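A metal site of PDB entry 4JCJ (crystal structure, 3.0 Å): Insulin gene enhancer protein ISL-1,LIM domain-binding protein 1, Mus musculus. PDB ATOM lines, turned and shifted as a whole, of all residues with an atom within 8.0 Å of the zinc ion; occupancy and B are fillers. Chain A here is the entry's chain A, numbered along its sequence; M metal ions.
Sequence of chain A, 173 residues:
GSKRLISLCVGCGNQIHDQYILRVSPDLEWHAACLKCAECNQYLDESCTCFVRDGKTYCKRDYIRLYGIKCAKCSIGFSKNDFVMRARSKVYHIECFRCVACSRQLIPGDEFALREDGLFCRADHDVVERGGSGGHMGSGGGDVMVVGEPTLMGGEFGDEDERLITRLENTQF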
ATOM      1  N   LYS A  70      14.470   7.246  21.930  1.00  0.00           N
ATOM      2  CA  LYS A  70      14.743   7.603  23.326  1.00  0.00           C
ATOM      3  C   LYS A  70      13.434   7.609  24.126  1.00  0.00           C
ATOM      4  O   LYS A  70      12.349   7.609  23.527  1.00  0.00           O
ATOM      5  CB  LYS A  70      15.432   8.973  23.400  1.00  0.00           C
ATOM      6  N   CYS A  71      13.522   7.637  25.453  1.00  0.00           N
ATOM      7  CA  CYS A  71      12.334   7.441  26.302  1.00  0.00           C
ATOM      8  C   CYS A  71      11.444   8.676  26.485  1.00  0.00           C
ATOM      9  O   CYS A  71      11.935   9.773  26.735  1.00  0.00           O
ATOM     10  CB  CYS A  71      12.737   6.940  27.674  1.00  0.00           C
ATOM     11  SG  CYS A  71      11.475   7.172  28.929  1.00  0.00           S
ATOM     12  N   ALA A  72      10.122   8.456  26.419  1.00  0.00           N
ATOM     13  CA  ALA A  72       9.122   9.530  26.394  1.00  0.00           C
ATOM     14  C   ALA A  72       9.018  10.291  27.713  1.00  0.00           C
ATOM     15  O   ALA A  72       8.583  11.441  27.733  1.00  0.00           O
ATOM     16  CB  ALA A  72       7.772   8.978  26.006  1.00  0.00           C
ATOM     17  N   LYS A  73       9.382   9.645  28.822  1.00  0.00           N
ATOM     18  CA  LYS A  73       9.514  10.340  30.087  1.00  0.00           C
ATOM     19  C   LYS A  73      10.888  11.018  30.149  1.00  0.00           C
ATOM     20  O   LYS A  73      11.025  12.192  29.779  1.00  0.00           O
ATOM     21  CB  LYS A  73       9.327   9.392  31.273  1.00  0.00           C
ATOM     22  N   CYS A  74      11.914  10.272  30.554  1.00  0.00           N
ATOM     23  CA  CYS A  74      13.188  10.863  30.976  1.00  0.00           C
ATOM     24  C   CYS A  74      14.054  11.412  29.832  1.00  0.00           C
ATOM     25  O   CYS A  74      15.115  12.001  30.086  1.00  0.00           O
ATOM     26  CB  CYS A  74      13.988   9.853  31.778  1.00  0.00           C
ATOM     27  SG  CYS A  74      14.512   8.444  30.798  1.00  0.00           S
ATOM     28  N   SER A  75      13.629  11.181  28.588  1.00  0.00           N
ATOM     29  CA  SER A  75      14.340  11.718  27.424  1.00  0.00           C
ATOM     30  C   SER A  75      15.791  11.225  27.389  1.00  0.00           C
ATOM     31  O   SER A  75      16.701  12.016  27.242  1.00  0.00           O
ATOM     32  CB  SER A  75      14.288  13.248  27.426  1.00  0.00           C
ATOM     33  OG  SER A  75      13.009  13.710  27.841  1.00  0.00           O
ATOM     34  N   ILE A  76      15.975   9.918  27.533  1.00  0.00           N
ATOM     35  CA  ILE A  76      17.312   9.302  27.490  1.00  0.00           C
ATOM     36  C   ILE A  76      17.260   8.005  26.668  1.00  0.00           C
ATOM     37  O   ILE A  76      16.356   7.193  26.827  1.00  0.00           O
ATOM     38  CB  ILE A  76      17.872   9.028  28.915  1.00  0.00           C
ATOM     39  N   GLY A  77      18.237   7.837  25.775  1.00  0.00           N
ATOM     40  CA  GLY A  77      18.290   6.704  24.860  1.00  0.00           C
ATOM     41  C   GLY A  77      18.340   5.354  25.536  1.00  0.00           C
ATOM     42  O   GLY A  77      18.470   5.259  26.765  1.00  0.00           O
ATOM     43  N   PHE A  78      18.241   4.281  24.731  1.00  0.00           N
ATOM     44  CA  PHE A  78      18.185   2.922  25.260  1.00  0.00           C
ATOM     45  C   PHE A  78      19.430   2.103  24.970  1.00  0.00           C
ATOM     46  O   PHE A  78      20.140   2.337  23.980  1.00  0.00           O
ATOM     47  CB  PHE A  78      16.981   2.200  24.699  1.00  0.00           C
ATOM     48  CG  PHE A  78      15.677   2.789  25.131  1.00  0.00           C
ATOM     49  CD1 PHE A  78      15.271   2.678  26.460  1.00  0.00           C
ATOM     50  CD2 PHE A  78      14.860   3.444  24.228  1.00  0.00           C
ATOM     51  CE1 PHE A  78      14.060   3.217  26.886  1.00  0.00           C
ATOM     52  CE2 PHE A  78      13.653   3.989  24.631  1.00  0.00           C
ATOM     53  CZ  PHE A  78      13.247   3.864  25.961  1.00  0.00           C
ATOM     54  N   VAL A  91       7.916   4.827  23.385  1.00  0.00           N
ATOM     55  CA  VAL A  91       8.594   3.794  24.173  1.00  0.00           C
ATOM     56  C   VAL A  91       8.973   4.350  25.561  1.00  0.00           C
ATOM     57  O   VAL A  91       9.103   5.561  25.739  1.00  0.00           O
ATOM     58  CB  VAL A  91       9.869   3.287  23.465  1.00  0.00           C
ATOM     59  N   TYR A  92       9.127   3.470  26.550  1.00  0.00           N
ATOM     60  CA  TYR A  92       9.392   3.875  27.915  1.00  0.00           C
ATOM     61  C   TYR A  92      10.280   2.868  28.656  1.00  0.00           C
ATOM     62  O   TYR A  92      10.018   1.661  28.586  1.00  0.00           O
ATOM     63  CB  TYR A  92       8.079   4.001  28.703  1.00  0.00           C
ATOM     64  CG  TYR A  92       7.186   5.177  28.339  1.00  0.00           C
ATOM     65  CD1 TYR A  92       7.343   6.414  28.960  1.00  0.00           C
ATOM     66  CD2 TYR A  92       6.143   5.036  27.429  1.00  0.00           C
ATOM     67  CE1 TYR A  92       6.511   7.492  28.665  1.00  0.00           C
ATOM     68  CE2 TYR A  92       5.294   6.112  27.123  1.00  0.00           C
ATOM     69  CZ  TYR A  92       5.485   7.337  27.749  1.00  0.00           C
ATOM     70  OH  TYR A  92       4.661   8.416  27.459  1.00  0.00           O
ATOM     71  N   HIS A  93      11.306   3.373  29.355  1.00  0.00           N
ATOM     72  CA  HIS A  93      12.063   2.613  30.363  1.00  0.00           C
ATOM     73  C   HIS A  93      11.133   1.899  31.305  1.00  0.00           C
ATOM     74  O   HIS A  93      10.268   2.549  31.919  1.00  0.00           O
ATOM     75  CB  HIS A  93      12.866   3.546  31.258  1.00  0.00           C
ATOM     76  CG  HIS A  93      14.065   4.152  30.616  1.00  0.00           C
ATOM     77  ND1 HIS A  93      14.049   5.413  30.066  1.00  0.00           N
ATOM     78  CD2 HIS A  93      15.323   3.681  30.451  1.00  0.00           C
ATOM     79  CE1 HIS A  93      15.253   5.694  29.576  1.00  0.00           C
ATOM     80  NE2 HIS A  93      16.043   4.659  29.800  1.00  0.00           N
ATOM     81  N   ILE A  94      11.327   0.596  31.507  1.00  0.00           N
ATOM     82  CA  ILE A  94      10.523  -0.165  32.465  1.00  0.00           C
ATOM     83  C   ILE A  94      10.458   0.578  33.802  1.00  0.00           C
ATOM     84  O   ILE A  94       9.405   0.607  34.450  1.00  0.00           O
ATOM     85  CB  ILE A  94      11.052  -1.586  32.689  1.00  0.00           C
ATOM     86  N   GLU A  95      11.561   1.207  34.203  1.00  0.00           N
ATOM     87  CA  GLU A  95      11.608   2.001  35.435  1.00  0.00           C
ATOM     88  C   GLU A  95      10.777   3.291  35.377  1.00  0.00           C
ATOM     89  O   GLU A  95      10.317   3.756  36.408  1.00  0.00           O
ATOM     90  CB  GLU A  95      13.062   2.331  35.793  1.00  0.00           C
ATOM     91  N   CYS A  96      10.588   3.859  34.181  1.00  0.00           N
ATOM     92  CA  CYS A  96       9.917   5.168  34.024  1.00  0.00           C
ATOM     93  C   CYS A  96       8.446   5.089  33.619  1.00  0.00           C
ATOM     94  O   CYS A  96       7.838   6.126  33.337  1.00  0.00           O
ATOM     95  CB  CYS A  96      10.576   6.019  32.943  1.00  0.00           C
ATOM     96  SG  CYS A  96      12.332   6.385  33.077  1.00  0.00           S
ATOM     97  N   PHE A  97       7.889   3.877  33.555  1.00  0.00           N
ATOM     98  CA  PHE A  97       6.504   3.718  33.123  1.00  0.00           C
ATOM     99  C   PHE A  97       5.559   3.967  34.300  1.00  0.00           C
ATOM    100  O   PHE A  97       4.887   3.054  34.778  1.00  0.00           O
ATOM    101  CB  PHE A  97       6.305   2.330  32.518  1.00  0.00           C
ATOM    102  CG  PHE A  97       5.119   2.235  31.580  1.00  0.00           C
ATOM    103  CD1 PHE A  97       5.060   3.020  30.443  1.00  0.00           C
ATOM    104  CD2 PHE A  97       4.092   1.335  31.828  1.00  0.00           C
ATOM    105  CE1 PHE A  97       3.980   2.915  29.584  1.00  0.00           C
ATOM    106  CE2 PHE A  97       3.024   1.223  30.969  1.00  0.00           C
ATOM    107  CZ  PHE A  97       2.958   2.009  29.845  1.00  0.00           C
HETATM  108 ZN    ZN M   1      12.763   6.939  30.866  1.00  0.00          ZN
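N of Lys 73 lies close to SG of Cys 71 (3.2 Å). N of Cys 71 is in hydrogen-bond range of O of Ile 76.
Four residues have an atom within 4 Å of the zinc ion: Cys 71, Cys 74, His 93 and Cys 96. The nearest printed residue that does not touch the zinc ion is Lys 73 (4.2 Å).
The zinc ion is bound by a ring nitrogen (ND1) of His 93 (2.1 Å), the side-chain sulfur of Cys 74 (2.3 Å), the side-chain sulfur of Cys 96 (2.3 Å) and the side-chain sulfur of Cys 71 (2.3 Å). The zinc ion has four donor atoms within binding distance.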
